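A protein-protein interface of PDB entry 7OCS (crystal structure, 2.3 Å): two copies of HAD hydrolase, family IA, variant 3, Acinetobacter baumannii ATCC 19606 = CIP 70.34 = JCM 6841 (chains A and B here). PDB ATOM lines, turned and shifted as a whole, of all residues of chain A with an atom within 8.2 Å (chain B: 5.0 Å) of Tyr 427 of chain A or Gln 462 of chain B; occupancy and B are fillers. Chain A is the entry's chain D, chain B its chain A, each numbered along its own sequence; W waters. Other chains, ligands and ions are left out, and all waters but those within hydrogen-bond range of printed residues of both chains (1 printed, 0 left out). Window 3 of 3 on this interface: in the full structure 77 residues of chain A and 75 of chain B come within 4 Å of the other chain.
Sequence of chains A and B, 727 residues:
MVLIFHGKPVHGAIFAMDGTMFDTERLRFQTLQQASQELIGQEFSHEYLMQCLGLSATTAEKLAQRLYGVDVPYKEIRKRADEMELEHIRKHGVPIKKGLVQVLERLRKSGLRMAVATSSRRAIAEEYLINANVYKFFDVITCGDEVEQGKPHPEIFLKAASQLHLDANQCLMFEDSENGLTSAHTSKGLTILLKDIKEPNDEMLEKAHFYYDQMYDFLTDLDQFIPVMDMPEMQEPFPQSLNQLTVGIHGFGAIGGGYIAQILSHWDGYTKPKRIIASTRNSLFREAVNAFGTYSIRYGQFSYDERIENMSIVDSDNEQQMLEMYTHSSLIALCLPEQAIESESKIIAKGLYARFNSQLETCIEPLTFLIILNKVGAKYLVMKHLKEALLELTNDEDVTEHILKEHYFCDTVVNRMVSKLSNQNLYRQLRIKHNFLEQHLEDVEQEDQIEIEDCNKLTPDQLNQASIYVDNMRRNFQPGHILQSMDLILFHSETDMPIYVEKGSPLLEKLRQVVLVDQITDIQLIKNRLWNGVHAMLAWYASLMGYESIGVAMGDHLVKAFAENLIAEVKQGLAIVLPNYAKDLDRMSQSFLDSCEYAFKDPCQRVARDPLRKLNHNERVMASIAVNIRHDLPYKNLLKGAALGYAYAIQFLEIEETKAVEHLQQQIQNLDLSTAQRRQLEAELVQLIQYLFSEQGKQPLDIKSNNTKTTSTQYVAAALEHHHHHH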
ATOM      1  N   LEU A 284     -33.510 -27.567  -9.105  1.00  0.00           N
ATOM      2  CA  LEU A 284     -32.639 -27.575 -10.272  1.00  0.00           C
ATOM      3  C   LEU A 284     -33.165 -28.578 -11.298  1.00  0.00           C
ATOM      4  O   LEU A 284     -33.224 -28.267 -12.477  1.00  0.00           O
ATOM      5  CB  LEU A 284     -31.197 -27.918  -9.867  1.00  0.00           C
ATOM      6  CG  LEU A 284     -30.187 -27.925 -11.002  1.00  0.00           C
ATOM      7  CD1 LEU A 284     -30.033 -26.538 -11.607  1.00  0.00           C
ATOM      8  CD2 LEU A 284     -28.858 -28.482 -10.544  1.00  0.00           C
ATOM      9  N   PHE A 285     -33.597 -29.761 -10.836  1.00  0.00           N
ATOM     10  CA  PHE A 285     -34.164 -30.782 -11.709  1.00  0.00           C
ATOM     11  C   PHE A 285     -35.527 -30.319 -12.235  1.00  0.00           C
ATOM     12  O   PHE A 285     -35.787 -30.410 -13.434  1.00  0.00           O
ATOM     13  CB  PHE A 285     -34.327 -32.107 -10.943  1.00  0.00           C
ATOM     14  CG  PHE A 285     -33.291 -33.150 -11.262  1.00  0.00           C
ATOM     15  CD1 PHE A 285     -31.983 -32.999 -10.843  1.00  0.00           C
ATOM     16  CD2 PHE A 285     -33.636 -34.306 -11.935  1.00  0.00           C
ATOM     17  CE1 PHE A 285     -31.030 -33.964 -11.135  1.00  0.00           C
ATOM     18  CE2 PHE A 285     -32.683 -35.268 -12.224  1.00  0.00           C
ATOM     19  CZ  PHE A 285     -31.386 -35.094 -11.818  1.00  0.00           C
ATOM     20  N   LEU A 421     -28.873 -38.327 -12.089  1.00  0.00           N
ATOM     21  CA  LEU A 421     -27.711 -37.489 -12.372  1.00  0.00           C
ATOM     22  C   LEU A 421     -27.445 -36.567 -11.184  1.00  0.00           C
ATOM     23  O   LEU A 421     -28.390 -36.058 -10.576  1.00  0.00           O
ATOM     24  CB  LEU A 421     -27.935 -36.655 -13.635  1.00  0.00           C
ATOM     25  CG  LEU A 421     -26.691 -36.004 -14.199  1.00  0.00           C
ATOM     26  CD1 LEU A 421     -25.757 -37.037 -14.767  1.00  0.00           C
ATOM     27  CD2 LEU A 421     -27.037 -34.992 -15.232  1.00  0.00           C
ATOM     28  N   SER A 422     -26.169 -36.373 -10.831  1.00  0.00           N
ATOM     29  CA  SER A 422     -25.817 -35.476  -9.737  1.00  0.00           C
ATOM     30  C   SER A 422     -26.098 -34.015 -10.135  1.00  0.00           C
ATOM     31  O   SER A 422     -26.160 -33.696 -11.329  1.00  0.00           O
ATOM     32  CB  SER A 422     -24.350 -35.651  -9.347  1.00  0.00           C
ATOM     33  OG  SER A 422     -23.473 -35.072 -10.297  1.00  0.00           O
ATOM     34  N   ASN A 423     -26.272 -33.132  -9.137  1.00  0.00           N
ATOM     35  CA  ASN A 423     -26.546 -31.715  -9.396  1.00  0.00           C
ATOM     36  C   ASN A 423     -25.357 -31.008 -10.032  1.00  0.00           C
ATOM     37  O   ASN A 423     -25.549 -30.092 -10.831  1.00  0.00           O
ATOM     38  CB  ASN A 423     -26.979 -31.015  -8.126  1.00  0.00           C
ATOM     39  CG  ASN A 423     -28.242 -31.588  -7.566  1.00  0.00           C
ATOM     40  OD1 ASN A 423     -29.316 -31.458  -8.147  1.00  0.00           O
ATOM     41  ND2 ASN A 423     -28.138 -32.265  -6.432  1.00  0.00           N
ATOM     42  N   GLN A 424     -24.122 -31.454  -9.703  1.00  0.00           N
ATOM     43  CA  GLN A 424     -22.895 -30.906 -10.289  1.00  0.00           C
ATOM     44  C   GLN A 424     -22.802 -31.305 -11.766  1.00  0.00           C
ATOM     45  O   GLN A 424     -22.499 -30.462 -12.612  1.00  0.00           O
ATOM     46  CB  GLN A 424     -21.651 -31.397  -9.517  1.00  0.00           C
ATOM     47  CG  GLN A 424     -21.358 -30.586  -8.247  1.00  0.00           C
ATOM     48  CD  GLN A 424     -20.088 -31.046  -7.538  1.00  0.00           C
ATOM     49  OE1 GLN A 424     -19.268 -31.806  -8.081  1.00  0.00           O
ATOM     50  NE2 GLN A 424     -19.898 -30.587  -6.306  1.00  0.00           N
ATOM     51  N   ASN A 425     -23.114 -32.570 -12.084  1.00  0.00           N
ATOM     52  CA  ASN A 425     -23.098 -33.028 -13.478  1.00  0.00           C
ATOM     53  C   ASN A 425     -24.215 -32.378 -14.290  1.00  0.00           C
ATOM     54  O   ASN A 425     -24.026 -32.099 -15.473  1.00  0.00           O
ATOM     55  CB  ASN A 425     -23.181 -34.542 -13.562  1.00  0.00           C
ATOM     56  CG  ASN A 425     -21.868 -35.218 -13.266  1.00  0.00           C
ATOM     57  OD1 ASN A 425     -20.793 -34.623 -13.400  1.00  0.00           O
ATOM     58  ND2 ASN A 425     -21.929 -36.469 -12.850  1.00  0.00           N
ATOM     59  N   LEU A 426     -25.371 -32.115 -13.651  1.00  0.00           N
ATOM     60  CA  LEU A 426     -26.470 -31.429 -14.307  1.00  0.00           C
ATOM     61  C   LEU A 426     -26.087 -29.978 -14.577  1.00  0.00           C
ATOM     62  O   LEU A 426     -26.369 -29.471 -15.650  1.00  0.00           O
ATOM     63  CB  LEU A 426     -27.756 -31.507 -13.459  1.00  0.00           C
ATOM     64  CG  LEU A 426     -28.980 -30.746 -14.010  1.00  0.00           C
ATOM     65  CD1 LEU A 426     -29.321 -31.187 -15.439  1.00  0.00           C
ATOM     66  CD2 LEU A 426     -30.176 -30.948 -13.128  1.00  0.00           C
ATOM     67  N   TYR A 427     -25.385 -29.331 -13.633  1.00  0.00           N
ATOM     68  CA  TYR A 427     -24.930 -27.955 -13.818  1.00  0.00           C
ATOM     69  C   TYR A 427     -23.975 -27.858 -15.015  1.00  0.00           C
ATOM     70  O   TYR A 427     -24.099 -26.936 -15.822  1.00  0.00           O
ATOM     71  CB  TYR A 427     -24.260 -27.405 -12.530  1.00  0.00           C
ATOM     72  CG  TYR A 427     -23.627 -26.042 -12.729  1.00  0.00           C
ATOM     73  CD1 TYR A 427     -24.407 -24.899 -12.819  1.00  0.00           C
ATOM     74  CD2 TYR A 427     -22.259 -25.910 -12.914  1.00  0.00           C
ATOM     75  CE1 TYR A 427     -23.839 -23.657 -13.066  1.00  0.00           C
ATOM     76  CE2 TYR A 427     -21.679 -24.672 -13.157  1.00  0.00           C
ATOM     77  CZ  TYR A 427     -22.474 -23.547 -13.236  1.00  0.00           C
ATOM     78  OH  TYR A 427     -21.906 -22.315 -13.464  1.00  0.00           O
ATOM     79  N   ARG A 428     -23.027 -28.810 -15.134  1.00  0.00           N
ATOM     80  CA  ARG A 428     -22.084 -28.817 -16.264  1.00  0.00           C
ATOM     81  C   ARG A 428     -22.849 -28.983 -17.584  1.00  0.00           C
ATOM     82  O   ARG A 428     -22.576 -28.276 -18.555  1.00  0.00           O
ATOM     83  CB  ARG A 428     -21.028 -29.940 -16.098  1.00  0.00           C
ATOM     84  CG  ARG A 428     -20.191 -30.192 -17.368  1.00  0.00           C
ATOM     85  CD  ARG A 428     -19.034 -31.122 -17.128  1.00  0.00           C
ATOM     86  NE  ARG A 428     -19.484 -32.454 -16.735  1.00  0.00           N
ATOM     87  CZ  ARG A 428     -18.678 -33.412 -16.283  1.00  0.00           C
ATOM     88  NH1 ARG A 428     -19.170 -34.594 -15.942  1.00  0.00           N
ATOM     89  NH2 ARG A 428     -17.371 -33.191 -16.170  1.00  0.00           N
ATOM     90  N   GLN A 429     -23.832 -29.885 -17.592  1.00  0.00           N
ATOM     91  CA  GLN A 429     -24.660 -30.137 -18.756  1.00  0.00           C
ATOM     92  C   GLN A 429     -25.439 -28.897 -19.150  1.00  0.00           C
ATOM     93  O   GLN A 429     -25.460 -28.544 -20.324  1.00  0.00           O
ATOM     94  CB  GLN A 429     -25.610 -31.301 -18.502  1.00  0.00           C
ATOM     95  CG  GLN A 429     -26.403 -31.683 -19.751  1.00  0.00           C
ATOM     96  CD  GLN A 429     -27.395 -32.801 -19.542  1.00  0.00           C
ATOM     97  OE1 GLN A 429     -28.230 -33.066 -20.400  1.00  0.00           O
ATOM     98  NE2 GLN A 429     -27.319 -33.492 -18.413  1.00  0.00           N
ATOM     99  N   LEU A 430     -26.043 -28.199 -18.160  1.00  0.00           N
ATOM    100  CA  LEU A 430     -26.786 -26.977 -18.402  1.00  0.00           C
ATOM    101  C   LEU A 430     -25.875 -25.905 -18.978  1.00  0.00           C
ATOM    102  O   LEU A 430     -26.272 -25.202 -19.888  1.00  0.00           O
ATOM    103  CB  LEU A 430     -27.441 -26.478 -17.105  1.00  0.00           C
ATOM    104  CG  LEU A 430     -28.610 -27.318 -16.595  1.00  0.00           C
ATOM    105  CD1 LEU A 430     -29.027 -26.883 -15.207  1.00  0.00           C
ATOM    106  CD2 LEU A 430     -29.782 -27.263 -17.555  1.00  0.00           C
ATOM    107  N   ARG A 431     -24.649 -25.796 -18.463  1.00  0.00           N
ATOM    108  CA  ARG A 431     -23.673 -24.828 -18.953  1.00  0.00           C
ATOM    109  C   ARG A 431     -23.259 -25.112 -20.421  1.00  0.00           C
ATOM    110  O   ARG A 431     -23.176 -24.184 -21.226  1.00  0.00           O
ATOM    111  CB  ARG A 431     -22.439 -24.802 -18.034  1.00  0.00           C
ATOM    112  CG  ARG A 431     -21.339 -23.853 -18.519  1.00  0.00           C
ATOM    113  CD  ARG A 431     -20.099 -23.854 -17.635  1.00  0.00           C
ATOM    114  NE  ARG A 431     -19.661 -25.203 -17.253  1.00  0.00           N
ATOM    115  CZ  ARG A 431     -18.953 -26.014 -18.037  1.00  0.00           C
ATOM    116  NH1 ARG A 431     -18.618 -25.636 -19.267  1.00  0.00           N
ATOM    117  NH2 ARG A 431     -18.580 -27.208 -17.602  1.00  0.00           N
ATOM    118  N   ILE A 432     -23.013 -26.391 -20.760  1.00  0.00           N
ATOM    119  CA  ILE A 432     -22.634 -26.767 -22.122  1.00  0.00           C
ATOM    120  C   ILE A 432     -23.811 -26.588 -23.106  1.00  0.00           C
ATOM    121  O   ILE A 432     -23.625 -26.004 -24.169  1.00  0.00           O
ATOM    122  CB  ILE A 432     -22.037 -28.207 -22.158  1.00  0.00           C
ATOM    123  CG1 ILE A 432     -20.745 -28.272 -21.334  1.00  0.00           C
ATOM    124  CG2 ILE A 432     -21.800 -28.678 -23.599  1.00  0.00           C
ATOM    125  CD1 ILE A 432     -20.225 -29.644 -21.113  1.00  0.00           C
ATOM    126  N   LYS A 433     -25.030 -27.036 -22.720  1.00  0.00           N
ATOM    127  CA  LYS A 433     -26.214 -26.906 -23.576  1.00  0.00           C
ATOM    128  C   LYS A 433     -26.673 -25.442 -23.709  1.00  0.00           C
ATOM    129  O   LYS A 433     -27.205 -25.069 -24.757  1.00  0.00           O
ATOM    130  CB  LYS A 433     -27.382 -27.790 -23.079  1.00  0.00           C
ATOM    131  CG  LYS A 433     -27.027 -29.263 -22.835  1.00  0.00           C
ATOM    132  CD  LYS A 433     -26.511 -29.977 -24.070  1.00  0.00           C
ATOM    133  CE  LYS A 433     -26.113 -31.414 -23.753  1.00  0.00           C
ATOM    134  NZ  LYS A 433     -27.267 -32.221 -23.254  1.00  0.00           N
ATOM    135  N   HIS A 434     -26.481 -24.609 -22.650  1.00  0.00           N
ATOM    136  CA  HIS A 434     -26.848 -23.193 -22.736  1.00  0.00           C
ATOM    137  C   HIS A 434     -25.953 -22.501 -23.748  1.00  0.00           C
ATOM    138  O   HIS A 434     -26.419 -21.647 -24.503  1.00  0.00           O
ATOM    139  CB  HIS A 434     -26.754 -22.482 -21.362  1.00  0.00           C
ATOM    140  CG  HIS A 434     -26.934 -20.982 -21.443  1.00  0.00           C
ATOM    141  ND1 HIS A 434     -28.188 -20.398 -21.362  1.00  0.00           N
ATOM    142  CD2 HIS A 434     -26.015 -20.010 -21.658  1.00  0.00           C
ATOM    143  CE1 HIS A 434     -27.989 -19.098 -21.509  1.00  0.00           C
ATOM    144  NE2 HIS A 434     -26.701 -18.816 -21.691  1.00  0.00           N
ATOM    145  N   LEU A 488     -32.001 -33.528 -22.596  1.00  0.00           N
ATOM    146  CA  LEU A 488     -31.669 -33.175 -21.225  1.00  0.00           C
ATOM    147  C   LEU A 488     -31.524 -34.474 -20.437  1.00  0.00           C
ATOM    148  O   LEU A 488     -32.507 -34.992 -19.909  1.00  0.00           O
ATOM    149  CB  LEU A 488     -32.753 -32.289 -20.604  1.00  0.00           C
ATOM    150  CG  LEU A 488     -32.520 -31.900 -19.146  1.00  0.00           C
ATOM    151  CD1 LEU A 488     -31.264 -31.067 -18.995  1.00  0.00           C
ATOM    152  CD2 LEU A 488     -33.714 -31.187 -18.581  1.00  0.00           C
ATOM    153  N   LEU A 490     -31.054 -36.907 -17.637  1.00  0.00           N
ATOM    154  CA  LEU A 490     -31.202 -36.844 -16.187  1.00  0.00           C
ATOM    155  C   LEU A 490     -30.953 -38.158 -15.483  1.00  0.00           C
ATOM    156  O   LEU A 490     -30.729 -38.152 -14.278  1.00  0.00           O
ATOM    157  CB  LEU A 490     -32.578 -36.293 -15.791  1.00  0.00           C
ATOM    158  CG  LEU A 490     -32.851 -34.819 -16.131  1.00  0.00           C
ATOM    159  CD1 LEU A 490     -34.144 -34.382 -15.549  1.00  0.00           C
ATOM    160  CD2 LEU A 490     -31.737 -33.908 -15.628  1.00  0.00           C
ATOM    161  N   LYS B 457     -26.608 -28.653  -3.491  1.00  0.00           N
ATOM    162  CA  LYS B 457     -25.206 -29.072  -3.446  1.00  0.00           C
ATOM    163  C   LYS B 457     -24.331 -28.251  -4.419  1.00  0.00           C
ATOM    164  O   LYS B 457     -23.345 -28.764  -4.955  1.00  0.00           O
ATOM    165  CB  LYS B 457     -25.076 -30.578  -3.730  1.00  0.00           C
ATOM    166  CG  LYS B 457     -23.931 -31.236  -2.963  1.00  0.00           C
ATOM    167  CD  LYS B 457     -23.684 -32.673  -3.407  1.00  0.00           C
ATOM    168  CE  LYS B 457     -24.684 -33.641  -2.815  1.00  0.00           C
ATOM    169  NZ  LYS B 457     -24.421 -35.041  -3.257  1.00  0.00           N
ATOM    170  N   LEU B 458     -24.687 -26.978  -4.639  1.00  0.00           N
ATOM    171  CA  LEU B 458     -23.912 -26.102  -5.521  1.00  0.00           C
ATOM    172  C   LEU B 458     -23.495 -24.824  -4.791  1.00  0.00           C
ATOM    173  O   LEU B 458     -24.187 -24.390  -3.868  1.00  0.00           O
ATOM    174  CB  LEU B 458     -24.728 -25.731  -6.774  1.00  0.00           C
ATOM    175  CG  LEU B 458     -25.220 -26.895  -7.624  1.00  0.00           C
ATOM    176  CD1 LEU B 458     -26.156 -26.412  -8.708  1.00  0.00           C
ATOM    177  CD2 LEU B 458     -24.065 -27.660  -8.221  1.00  0.00           C
ATOM    178  N   THR B 459     -22.383 -24.201  -5.219  1.00  0.00           N
ATOM    179  CA  THR B 459     -21.944 -22.926  -4.637  1.00  0.00           C
ATOM    180  C   THR B 459     -22.945 -21.822  -5.046  1.00  0.00           C
ATOM    181  O   THR B 459     -23.504 -21.885  -6.141  1.00  0.00           O
ATOM    182  CB  THR B 459     -20.486 -22.581  -5.081  1.00  0.00           C
ATOM    183  OG1 THR B 459     -20.485 -22.066  -6.418  1.00  0.00           O
ATOM    184  CG2 THR B 459     -19.537 -23.772  -4.968  1.00  0.00           C
ATOM    185  N   PRO B 460     -23.189 -20.805  -4.192  1.00  0.00           N
ATOM    186  CA  PRO B 460     -24.155 -19.749  -4.570  1.00  0.00           C
ATOM    187  C   PRO B 460     -23.802 -19.046  -5.880  1.00  0.00           C
ATOM    188  O   PRO B 460     -24.695 -18.640  -6.615  1.00  0.00           O
ATOM    189  CB  PRO B 460     -24.114 -18.786  -3.378  1.00  0.00           C
ATOM    190  CG  PRO B 460     -23.604 -19.608  -2.241  1.00  0.00           C
ATOM    191  CD  PRO B 460     -22.635 -20.577  -2.844  1.00  0.00           C
ATOM    192  N   ASP B 461     -22.503 -18.936  -6.186  1.00  0.00           N
ATOM    193  CA  ASP B 461     -22.014 -18.317  -7.416  1.00  0.00           C
ATOM    194  C   ASP B 461     -22.499 -19.095  -8.647  1.00  0.00           C
ATOM    195  O   ASP B 461     -22.938 -18.483  -9.628  1.00  0.00           O
ATOM    196  CB  ASP B 461     -20.469 -18.243  -7.389  1.00  0.00           C
ATOM    197  CG  ASP B 461     -19.828 -17.697  -8.655  1.00  0.00           C
ATOM    198  OD1 ASP B 461     -20.502 -16.921  -9.379  1.00  0.00           O
ATOM    199  OD2 ASP B 461     -18.647 -18.035  -8.917  1.00  0.00           O
ATOM    200  N   GLN B 462     -22.429 -20.435  -8.600  1.00  0.00           N
ATOM    201  CA  GLN B 462     -22.870 -21.242  -9.730  1.00  0.00           C
ATOM    202  C   GLN B 462     -24.380 -21.546  -9.689  1.00  0.00           C
ATOM    203  O   GLN B 462     -24.975 -21.761 -10.731  1.00  0.00           O
ATOM    204  CB  GLN B 462     -22.022 -22.511  -9.887  1.00  0.00           C
ATOM    205  CG  GLN B 462     -22.272 -23.589  -8.843  1.00  0.00           C
ATOM    206  CD  GLN B 462     -21.193 -24.668  -8.854  1.00  0.00           C
ATOM    207  OE1 GLN B 462     -20.300 -24.704  -9.716  1.00  0.00           O
ATOM    208  NE2 GLN B 462     -21.255 -25.567  -7.894  1.00  0.00           N
ATOM    209  N   LEU B 463     -25.008 -21.470  -8.504  1.00  0.00           N
ATOM    210  CA  LEU B 463     -26.454 -21.658  -8.364  1.00  0.00           C
ATOM    211  C   LEU B 463     -27.210 -20.463  -9.008  1.00  0.00           C
ATOM    212  O   LEU B 463     -28.298 -20.641  -9.548  1.00  0.00           O
ATOM    213  CB  LEU B 463     -26.826 -21.790  -6.883  1.00  0.00           C
ATOM    214  CG  LEU B 463     -28.187 -22.396  -6.596  1.00  0.00           C
ATOM    215  CD1 LEU B 463     -28.226 -23.838  -6.991  1.00  0.00           C
ATOM    216  CD2 LEU B 463     -28.535 -22.264  -5.139  1.00  0.00           C
ATOM    217  N   ASN B 464     -26.621 -19.258  -8.954  1.00  0.00           N
ATOM    218  CA  ASN B 464     -27.205 -18.085  -9.599  1.00  0.00           C
ATOM    219  C   ASN B 464     -26.962 -18.153 -11.118  1.00  0.00           C
ATOM    220  O   ASN B 464     -27.823 -17.751 -11.895  1.00  0.00           O
ATOM    221  CB  ASN B 464     -26.614 -16.796  -9.020  1.00  0.00           C
ATOM    222  CG  ASN B 464     -27.223 -15.542  -9.605  1.00  0.00           C
ATOM    223  OD1 ASN B 464     -28.438 -15.306  -9.513  1.00  0.00           O
ATOM    224  ND2 ASN B 464     -26.394 -14.711 -10.231  1.00  0.00           N
ATOM    225  N   GLN B 465     -25.790 -18.679 -11.529  1.00  0.00           N
ATOM    226  CA  GLN B 465     -25.413 -18.868 -12.927  1.00  0.00           C
ATOM    227  C   GLN B 465     -26.358 -19.880 -13.597  1.00  0.00           C
ATOM    228  O   GLN B 465     -26.790 -19.666 -14.725  1.00  0.00           O
ATOM    229  CB  GLN B 465     -23.967 -19.362 -13.005  1.00  0.00           C
ATOM    230  CG  GLN B 465     -23.417 -19.399 -14.403  1.00  0.00           C
ATOM    231  CD  GLN B 465     -23.031 -18.036 -14.895  1.00  0.00           C
ATOM    232  OE1 GLN B 465     -22.067 -17.426 -14.418  1.00  0.00           O
ATOM    233  NE2 GLN B 465     -23.767 -17.528 -15.877  1.00  0.00           N
ATOM    234  N   ALA B 466     -26.717 -20.956 -12.866  1.00  0.00           N
ATOM    235  CA  ALA B 466     -27.644 -21.982 -13.331  1.00  0.00           C
ATOM    236  C   ALA B 466     -29.040 -21.396 -13.518  1.00  0.00           C
ATOM    237  O   ALA B 466     -29.721 -21.733 -14.485  1.00  0.00           O
ATOM    238  CB  ALA B 466     -27.694 -23.127 -12.339  1.00  0.00           C
ATOM    239  N   TYR B 469     -29.065 -19.730 -16.873  1.00  0.00           N
ATOM    240  CA  TYR B 469     -29.109 -20.749 -17.933  1.00  0.00           C
ATOM    241  C   TYR B 469     -30.545 -21.261 -18.118  1.00  0.00           C
ATOM    242  O   TYR B 469     -31.083 -21.201 -19.219  1.00  0.00           O
ATOM    243  CB  TYR B 469     -28.184 -21.949 -17.586  1.00  0.00           C
ATOM    244  CG  TYR B 469     -26.710 -21.624 -17.501  1.00  0.00           C
ATOM    245  CD1 TYR B 469     -26.153 -20.619 -18.277  1.00  0.00           C
ATOM    246  CD2 TYR B 469     -25.860 -22.362 -16.687  1.00  0.00           C
ATOM    247  CE1 TYR B 469     -24.796 -20.332 -18.221  1.00  0.00           C
ATOM    248  CE2 TYR B 469     -24.501 -22.087 -16.625  1.00  0.00           C
ATOM    249  CZ  TYR B 469     -23.968 -21.080 -17.407  1.00  0.00           C
ATOM    250  OH  TYR B 469     -22.624 -20.799 -17.354  1.00  0.00           O
HETATM  251  O   HOH W   1     -26.017 -34.384  -5.973  1.00  0.00           O
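Phe 285 of chain A touches none of the printed residues of chain B. Ser 422 of chain A touches none of the printed residues of chain B. Of the printed residues of chain B, Gln 424 of chain A touches Leu 458. Of chain B, only Gln 462 (3.2 Å), Gln 465 (3.4 Å), Ala 466 (3.8 Å) and Tyr 469 (3.9 Å) come within 4 Å of Tyr 427 of chain A. Of the printed residues of chain B, His 434 of chain A touches Tyr 469 (3.3 Å). Printed residues of chain A within 4 Å of Leu 458 of chain B: Leu 284 (3.9 Å), Asn 423 (3.9 Å) and Gln 424 (3.99 Å). Gln 462 of chain B touches just one residue of chain A: Tyr 427. Of the printed residues of chain A, Ala 466 of chain B touches Tyr 427. The nearest residue of chain A that does not touch Gln 462 of chain B is Gln 424 of chain A (5.0 Å).
No position is printed for both chains.
N of Thr 459 of chain B lies close to NE2 of Gln 462 of chain B, at 3.2 Å.
Water W1 lies within hydrogen-bond range of ND2 of Asn 423 of chain A (3.0 Å) and NZ of Lys 457 of chain B (3.2 Å).
Of the 18 printed residues of chain A, 6 touch a printed residue of chain B. Hydrophobic or aromatic side chains of chain B that line the printed part of chain A: Leu 458, Ala 466 and Tyr 469. Among the printed residues, no Asp or Glu carboxylate lies within 4 Å of a Lys or Arg side-chain nitrogen of the other chain.
CD2 of Leu 284 of chain A touches CD1 of Leu 458 of chain B, at 3.9 Å. Leu 458 of chain B touches Asn 423 of chain A. Leu 458 of chain B touches Gln 424 of chain A. Tyr 427 of chain A touches Gln 462 of chain B. Tyr 427 of chain A touches Gln 465 of chain B. Tyr 427 of chain A touches Ala 466 of chain B. Tyr 427 of chain A touches Tyr 469 of chain B. Arg 431 of chain A touches Tyr 469 of chain B (CG to OH, 3.5 Å). His 434 of chain A touches Tyr 469 of chain B.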
